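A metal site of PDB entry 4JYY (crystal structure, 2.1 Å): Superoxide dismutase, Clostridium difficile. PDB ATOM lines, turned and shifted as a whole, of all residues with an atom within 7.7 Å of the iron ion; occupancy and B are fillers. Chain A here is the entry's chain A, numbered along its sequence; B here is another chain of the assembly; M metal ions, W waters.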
ATOM      1  N   HIS A  30       4.910  14.567 -22.458  1.00  0.00           N
ATOM      2  CA  HIS A  30       5.601  13.324 -22.201  1.00  0.00           C
ATOM      3  C   HIS A  30       4.746  12.440 -21.298  1.00  0.00           C
ATOM      4  O   HIS A  30       4.564  11.253 -21.568  1.00  0.00           O
ATOM      5  CB  HIS A  30       6.930  13.645 -21.540  1.00  0.00           C
ATOM      6  CG  HIS A  30       7.950  12.563 -21.676  1.00  0.00           C
ATOM      7  ND1 HIS A  30       9.202  12.672 -21.102  1.00  0.00           N
ATOM      8  CD2 HIS A  30       7.917  11.368 -22.305  1.00  0.00           C
ATOM      9  CE1 HIS A  30       9.902  11.586 -21.382  1.00  0.00           C
ATOM     10  NE2 HIS A  30       9.139  10.779 -22.097  1.00  0.00           N
ATOM     11  N   HIS A  31       4.179  13.031 -20.248  1.00  0.00           N
ATOM     12  CA  HIS A  31       3.348  12.275 -19.327  1.00  0.00           C
ATOM     13  C   HIS A  31       1.936  12.082 -19.854  1.00  0.00           C
ATOM     14  O   HIS A  31       1.418  10.963 -19.882  1.00  0.00           O
ATOM     15  CB  HIS A  31       3.306  12.944 -17.942  1.00  0.00           C
ATOM     16  CG  HIS A  31       2.438  12.238 -16.943  1.00  0.00           C
ATOM     17  ND1 HIS A  31       1.068  12.348 -16.941  1.00  0.00           N
ATOM     18  CD2 HIS A  31       2.750  11.415 -15.915  1.00  0.00           C
ATOM     19  CE1 HIS A  31       0.571  11.620 -15.957  1.00  0.00           C
ATOM     20  NE2 HIS A  31       1.575  11.051 -15.306  1.00  0.00           N
ATOM     21  N   HIS A  34       2.393  10.793 -24.374  1.00  0.00           N
ATOM     22  CA  HIS A  34       3.193   9.612 -24.696  1.00  0.00           C
ATOM     23  C   HIS A  34       2.969   8.471 -23.689  1.00  0.00           C
ATOM     24  O   HIS A  34       2.600   7.360 -24.058  1.00  0.00           O
ATOM     25  CB  HIS A  34       4.681   9.979 -24.781  1.00  0.00           C
ATOM     26  CG  HIS A  34       5.004  10.919 -25.900  1.00  0.00           C
ATOM     27  ND1 HIS A  34       5.150  10.495 -27.208  1.00  0.00           N
ATOM     28  CD2 HIS A  34       5.181  12.257 -25.923  1.00  0.00           C
ATOM     29  CE1 HIS A  34       5.436  11.523 -27.973  1.00  0.00           C
ATOM     30  NE2 HIS A  34       5.455  12.610 -27.228  1.00  0.00           N
ATOM     31  N   TYR A  35       3.205   8.746 -22.416  1.00  0.00           N
ATOM     32  CA  TYR A  35       3.018   7.717 -21.388  1.00  0.00           C
ATOM     33  C   TYR A  35       1.584   7.200 -21.438  1.00  0.00           C
ATOM     34  O   TYR A  35       1.349   5.987 -21.471  1.00  0.00           O
ATOM     35  CB  TYR A  35       3.409   8.298 -20.012  1.00  0.00           C
ATOM     36  CG  TYR A  35       3.190   7.425 -18.787  1.00  0.00           C
ATOM     37  CD1 TYR A  35       3.071   6.037 -18.865  1.00  0.00           C
ATOM     38  CD2 TYR A  35       3.148   8.006 -17.525  1.00  0.00           C
ATOM     39  CE1 TYR A  35       2.887   5.259 -17.709  1.00  0.00           C
ATOM     40  CE2 TYR A  35       2.963   7.265 -16.371  1.00  0.00           C
ATOM     41  CZ  TYR A  35       2.829   5.889 -16.466  1.00  0.00           C
ATOM     42  OH  TYR A  35       2.655   5.187 -15.293  1.00  0.00           O
ATOM     43  N   TYR A  38       0.959   4.641 -24.285  1.00  0.00           N
ATOM     44  CA  TYR A  38       1.482   3.301 -24.014  1.00  0.00           C
ATOM     45  C   TYR A  38       0.513   2.496 -23.166  1.00  0.00           C
ATOM     46  O   TYR A  38       0.217   1.342 -23.457  1.00  0.00           O
ATOM     47  CB  TYR A  38       2.860   3.359 -23.357  1.00  0.00           C
ATOM     48  CG  TYR A  38       3.928   3.889 -24.291  1.00  0.00           C
ATOM     49  CD1 TYR A  38       4.127   3.321 -25.552  1.00  0.00           C
ATOM     50  CD2 TYR A  38       4.730   4.955 -23.906  1.00  0.00           C
ATOM     51  CE1 TYR A  38       5.111   3.807 -26.418  1.00  0.00           C
ATOM     52  CE2 TYR A  38       5.715   5.445 -24.758  1.00  0.00           C
ATOM     53  CZ  TYR A  38       5.891   4.872 -26.009  1.00  0.00           C
ATOM     54  OH  TYR A  38       6.885   5.361 -26.832  1.00  0.00           O
ATOM     55  N   GLY A  81       6.833   0.803 -22.720  1.00  0.00           N
ATOM     56  CA  GLY A  81       6.679   2.243 -22.620  1.00  0.00           C
ATOM     57  C   GLY A  81       6.050   2.625 -21.287  1.00  0.00           C
ATOM     58  O   GLY A  81       6.429   3.606 -20.674  1.00  0.00           O
ATOM     59  N   ASN A  84       8.703   1.963 -18.479  1.00  0.00           N
ATOM     60  CA  ASN A  84       9.854   2.845 -18.593  1.00  0.00           C
ATOM     61  C   ASN A  84       9.510   4.270 -18.154  1.00  0.00           C
ATOM     62  O   ASN A  84      10.309   4.935 -17.509  1.00  0.00           O
ATOM     63  CB  ASN A  84      10.395   2.855 -20.038  1.00  0.00           C
ATOM     64  CG  ASN A  84      11.084   1.554 -20.439  1.00  0.00           C
ATOM     65  OD1 ASN A  84      11.423   0.735 -19.575  1.00  0.00           O
ATOM     66  ND2 ASN A  84      11.293   1.353 -21.749  1.00  0.00           N
ATOM     67  N   HIS A  85       8.318   4.724 -18.506  1.00  0.00           N
ATOM     68  CA  HIS A  85       7.903   6.094 -18.186  1.00  0.00           C
ATOM     69  C   HIS A  85       7.506   6.259 -16.722  1.00  0.00           C
ATOM     70  O   HIS A  85       7.856   7.257 -16.097  1.00  0.00           O
ATOM     71  CB  HIS A  85       6.798   6.562 -19.133  1.00  0.00           C
ATOM     72  CG  HIS A  85       7.306   6.887 -20.500  1.00  0.00           C
ATOM     73  ND1 HIS A  85       7.606   5.914 -21.428  1.00  0.00           N
ATOM     74  CD2 HIS A  85       7.623   8.068 -21.079  1.00  0.00           C
ATOM     75  CE1 HIS A  85       8.068   6.475 -22.522  1.00  0.00           C
ATOM     76  NE2 HIS A  85       8.090   7.787 -22.344  1.00  0.00           N
ATOM     77  N   PHE A  88      10.782   6.446 -15.172  1.00  0.00           N
ATOM     78  CA  PHE A  88      11.515   7.665 -15.491  1.00  0.00           C
ATOM     79  C   PHE A  88      10.981   8.864 -14.704  1.00  0.00           C
ATOM     80  O   PHE A  88      11.753   9.647 -14.159  1.00  0.00           O
ATOM     81  CB  PHE A  88      11.416   7.933 -16.996  1.00  0.00           C
ATOM     82  CG  PHE A  88      12.205   9.131 -17.469  1.00  0.00           C
ATOM     83  CD1 PHE A  88      13.587   9.180 -17.306  1.00  0.00           C
ATOM     84  CD2 PHE A  88      11.578  10.186 -18.107  1.00  0.00           C
ATOM     85  CE1 PHE A  88      14.326  10.275 -17.756  1.00  0.00           C
ATOM     86  CE2 PHE A  88      12.298  11.290 -18.565  1.00  0.00           C
ATOM     87  CZ  PHE A  88      13.676  11.339 -18.380  1.00  0.00           C
ATOM     88  N   PHE A  89       9.669   9.025 -14.617  1.00  0.00           N
ATOM     89  CA  PHE A  89       9.162  10.173 -13.878  1.00  0.00           C
ATOM     90  C   PHE A  89       9.447  10.006 -12.375  1.00  0.00           C
ATOM     91  O   PHE A  89       9.723  10.996 -11.677  1.00  0.00           O
ATOM     92  CB  PHE A  89       7.684  10.426 -14.174  1.00  0.00           C
ATOM     93  CG  PHE A  89       7.391  10.713 -15.633  1.00  0.00           C
ATOM     94  CD1 PHE A  89       8.122  11.678 -16.321  1.00  0.00           C
ATOM     95  CD2 PHE A  89       6.399  10.027 -16.302  1.00  0.00           C
ATOM     96  CE1 PHE A  89       7.862  11.948 -17.668  1.00  0.00           C
ATOM     97  CE2 PHE A  89       6.129  10.288 -17.647  1.00  0.00           C
ATOM     98  CZ  PHE A  89       6.866  11.259 -18.329  1.00  0.00           C
ATOM     99  N   GLY A 132      15.663   5.447 -27.805  1.00  0.00           N
ATOM    100  CA  GLY A 132      16.014   4.504 -26.743  1.00  0.00           C
ATOM    101  C   GLY A 132      16.314   5.135 -25.395  1.00  0.00           C
ATOM    102  O   GLY A 132      15.963   6.285 -25.128  1.00  0.00           O
ATOM    103  N   TRP A 133      17.012   4.372 -24.565  1.00  0.00           N
ATOM    104  CA  TRP A 133      17.219   4.677 -23.143  1.00  0.00           C
ATOM    105  C   TRP A 133      18.634   4.336 -22.755  1.00  0.00           C
ATOM    106  O   TRP A 133      19.224   3.387 -23.287  1.00  0.00           O
ATOM    107  CB  TRP A 133      16.287   3.809 -22.304  1.00  0.00           C
ATOM    108  CG  TRP A 133      14.857   4.125 -22.481  1.00  0.00           C
ATOM    109  CD1 TRP A 133      14.049   3.749 -23.511  1.00  0.00           C
ATOM    110  CD2 TRP A 133      14.037   4.885 -21.578  1.00  0.00           C
ATOM    111  NE1 TRP A 133      12.787   4.233 -23.318  1.00  0.00           N
ATOM    112  CE2 TRP A 133      12.748   4.943 -22.147  1.00  0.00           C
ATOM    113  CE3 TRP A 133      14.272   5.530 -20.360  1.00  0.00           C
ATOM    114  CZ2 TRP A 133      11.686   5.620 -21.534  1.00  0.00           C
ATOM    115  CZ3 TRP A 133      13.223   6.191 -19.745  1.00  0.00           C
ATOM    116  CH2 TRP A 133      11.938   6.235 -20.340  1.00  0.00           C
ATOM    117  N   ASN A 151      14.269   1.782 -28.430  1.00  0.00           N
ATOM    118  CA  ASN A 151      12.822   1.950 -28.408  1.00  0.00           C
ATOM    119  C   ASN A 151      12.290   1.882 -26.964  1.00  0.00           C
ATOM    120  O   ASN A 151      12.721   2.683 -26.135  1.00  0.00           O
ATOM    121  CB  ASN A 151      12.192   0.944 -29.383  1.00  0.00           C
ATOM    122  CG  ASN A 151      12.780   1.088 -30.806  1.00  0.00           C
ATOM    123  OD1 ASN A 151      13.040   2.214 -31.280  1.00  0.00           O
ATOM    124  ND2 ASN A 151      13.026  -0.052 -31.470  1.00  0.00           N
ATOM    125  N   GLN A 152      11.373   0.965 -26.661  1.00  0.00           N
ATOM    126  CA  GLN A 152      10.916   0.818 -25.269  1.00  0.00           C
ATOM    127  C   GLN A 152      11.347  -0.508 -24.651  1.00  0.00           C
ATOM    128  O   GLN A 152      10.694  -1.024 -23.730  1.00  0.00           O
ATOM    129  CB  GLN A 152       9.389   0.970 -25.120  1.00  0.00           C
ATOM    130  CG  GLN A 152       8.843   2.338 -25.564  1.00  0.00           C
ATOM    131  CD  GLN A 152       9.413   3.522 -24.775  1.00  0.00           C
ATOM    132  OE1 GLN A 152       9.302   4.674 -25.220  1.00  0.00           O
ATOM    133  NE2 GLN A 152      10.048   3.251 -23.638  1.00  0.00           N
ATOM    134  N   ASP A 167      15.575   8.662 -20.641  1.00  0.00           N
ATOM    135  CA  ASP A 167      14.887   8.575 -21.920  1.00  0.00           C
ATOM    136  C   ASP A 167      15.593   9.473 -22.932  1.00  0.00           C
ATOM    137  O   ASP A 167      15.652  10.689 -22.726  1.00  0.00           O
ATOM    138  CB  ASP A 167      13.462   9.096 -21.716  1.00  0.00           C
ATOM    139  CG  ASP A 167      12.569   8.868 -22.908  1.00  0.00           C
ATOM    140  OD1 ASP A 167      13.044   8.495 -24.005  1.00  0.00           O
ATOM    141  OD2 ASP A 167      11.353   9.083 -22.747  1.00  0.00           O
ATOM    142  N   VAL A 168      16.144   8.903 -24.008  1.00  0.00           N
ATOM    143  CA  VAL A 168      16.703   9.747 -25.076  1.00  0.00           C
ATOM    144  C   VAL A 168      15.957   9.664 -26.425  1.00  0.00           C
ATOM    145  O   VAL A 168      16.523   9.965 -27.476  1.00  0.00           O
ATOM    146  CB  VAL A 168      18.227   9.568 -25.284  1.00  0.00           C
ATOM    147  CG1 VAL A 168      18.999  10.060 -24.046  1.00  0.00           C
ATOM    148  CG2 VAL A 168      18.575   8.114 -25.622  1.00  0.00           C
ATOM    149  N   TRP A 169      14.695   9.241 -26.380  1.00  0.00           N
ATOM    150  CA  TRP A 169      13.801   9.499 -27.494  1.00  0.00           C
ATOM    151  C   TRP A 169      13.791  11.017 -27.694  1.00  0.00           C
ATOM    152  O   TRP A 169      13.860  11.783 -26.706  1.00  0.00           O
ATOM    153  CB  TRP A 169      12.383   9.048 -27.190  1.00  0.00           C
ATOM    154  CG  TRP A 169      12.124   7.558 -27.262  1.00  0.00           C
ATOM    155  CD1 TRP A 169      12.758   6.571 -26.575  1.00  0.00           C
ATOM    156  CD2 TRP A 169      11.108   6.908 -28.055  1.00  0.00           C
ATOM    157  NE1 TRP A 169      12.220   5.344 -26.888  1.00  0.00           N
ATOM    158  CE2 TRP A 169      11.204   5.528 -27.786  1.00  0.00           C
ATOM    159  CE3 TRP A 169      10.135   7.365 -28.950  1.00  0.00           C
ATOM    160  CZ2 TRP A 169      10.357   4.590 -28.411  1.00  0.00           C
ATOM    161  CZ3 TRP A 169       9.300   6.439 -29.565  1.00  0.00           C
ATOM    162  CH2 TRP A 169       9.421   5.055 -29.282  1.00  0.00           C
ATOM    163  N   GLU A 170      13.694  11.453 -28.942  1.00  0.00           N
ATOM    164  CA  GLU A 170      13.717  12.877 -29.223  1.00  0.00           C
ATOM    165  C   GLU A 170      12.544  13.624 -28.583  1.00  0.00           C
ATOM    166  O   GLU A 170      12.696  14.765 -28.212  1.00  0.00           O
ATOM    167  CB  GLU A 170      13.854  13.142 -30.745  1.00  0.00           C
ATOM    168  CG  GLU A 170      15.266  12.845 -31.236  1.00  0.00           C
ATOM    169  CD  GLU A 170      15.418  12.831 -32.763  1.00  0.00           C
ATOM    170  OE1 GLU A 170      14.468  12.439 -33.450  1.00  0.00           O
ATOM    171  OE2 GLU A 170      16.493  13.215 -33.245  1.00  0.00           O
ATOM    172  N   HIS A 171      11.389  12.982 -28.433  1.00  0.00           N
ATOM    173  CA  HIS A 171      10.297  13.684 -27.759  1.00  0.00           C
ATOM    174  C   HIS A 171      10.637  14.114 -26.328  1.00  0.00           C
ATOM    175  O   HIS A 171       9.983  14.998 -25.782  1.00  0.00           O
ATOM    176  CB  HIS A 171       8.978  12.897 -27.788  1.00  0.00           C
ATOM    177  CG  HIS A 171       9.014  11.612 -27.019  1.00  0.00           C
ATOM    178  ND1 HIS A 171       8.669  10.395 -27.576  1.00  0.00           N
ATOM    179  CD2 HIS A 171       9.320  11.359 -25.723  1.00  0.00           C
ATOM    180  CE1 HIS A 171       8.764   9.450 -26.655  1.00  0.00           C
ATOM    181  NE2 HIS A 171       9.164  10.006 -25.523  1.00  0.00           N
ATOM    182  N   ALA A 172      11.656  13.495 -25.732  1.00  0.00           N
ATOM    183  CA  ALA A 172      12.016  13.801 -24.352  1.00  0.00           C
ATOM    184  C   ALA A 172      12.786  15.104 -24.249  1.00  0.00           C
ATOM    185  O   ALA A 172      12.893  15.671 -23.156  1.00  0.00           O
ATOM    186  CB  ALA A 172      12.838  12.655 -23.735  1.00  0.00           C
ATOM    187  N   TYR A 184      20.978  18.227 -22.936  1.00  0.00           N
ATOM    188  CA  TYR A 184      19.878  17.590 -22.222  1.00  0.00           C
ATOM    189  C   TYR A 184      20.408  16.574 -21.221  1.00  0.00           C
ATOM    190  O   TYR A 184      19.971  16.546 -20.057  1.00  0.00           O
ATOM    191  CB  TYR A 184      18.962  16.907 -23.219  1.00  0.00           C
ATOM    192  CG  TYR A 184      17.987  15.887 -22.646  1.00  0.00           C
ATOM    193  CD1 TYR A 184      16.980  16.276 -21.777  1.00  0.00           C
ATOM    194  CD2 TYR A 184      18.058  14.549 -23.028  1.00  0.00           C
ATOM    195  CE1 TYR A 184      16.067  15.361 -21.278  1.00  0.00           C
ATOM    196  CE2 TYR A 184      17.152  13.613 -22.532  1.00  0.00           C
ATOM    197  CZ  TYR A 184      16.173  14.025 -21.663  1.00  0.00           C
ATOM    198  OH  TYR A 184      15.265  13.123 -21.182  1.00  0.00           O
ATOM    199  N   GLU B 170      11.242  11.697 -34.685  1.00  0.00           N
ATOM    200  CA  GLU B 170      10.564  12.795 -34.015  1.00  0.00           C
ATOM    201  C   GLU B 170      11.191  14.150 -34.331  1.00  0.00           C
ATOM    202  O   GLU B 170      10.484  15.128 -34.390  1.00  0.00           O
ATOM    203  CB  GLU B 170      10.437  12.525 -32.500  1.00  0.00           C
ATOM    204  CG  GLU B 170       9.376  11.447 -32.213  1.00  0.00           C
ATOM    205  CD  GLU B 170       9.365  10.944 -30.773  1.00  0.00           C
ATOM    206  OE1 GLU B 170      10.427  10.878 -30.149  1.00  0.00           O
ATOM    207  OE2 GLU B 170       8.271  10.614 -30.274  1.00  0.00           O
HETATM  208 FE    FE M   1       9.556   8.999 -23.506  1.00  0.00          FE
HETATM  209  O   HOH W   1      10.438   7.152 -24.742  1.00  0.00           O
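The backbone NH of Trp 169 sits at hydrogen-bond distance from the side-chain carboxylate of Asp 167 (3.0 Å). O of Asp 167 sits at hydrogen-bond distance from OH of Tyr 184 (2.9 Å). ND1 of His 85 is in hydrogen-bond range of O of Gly 81, at 2.7 Å. The side-chain carboxylate of Glu 170 of chain B sits at hydrogen-bond distance from a ring nitrogen (ND1) of His 171, at 2.7 Å. O of His 30 lies within hydrogen-bond range of N of Tyr 35 (3.0 Å).
Within 4 Å of the iron ion: His 30, His 85, Asp 167 and His 171. The nearest printed residue that does not touch the iron ion is Trp 133 (4.5 Å).
The iron ion is bound by the side-chain carboxylate (OD2) of Asp 167, a ring nitrogen (NE2) of His 85, a ring nitrogen (NE2) of His 171, a ring nitrogen (NE2) of His 30 and water W1.
Water W1 lies within hydrogen-bond range of OE1 of Gln 152 (2.8 Å), OD1 of Asp 167 (3.0 Å) and NE1 of Trp 169 (3.3 Å).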
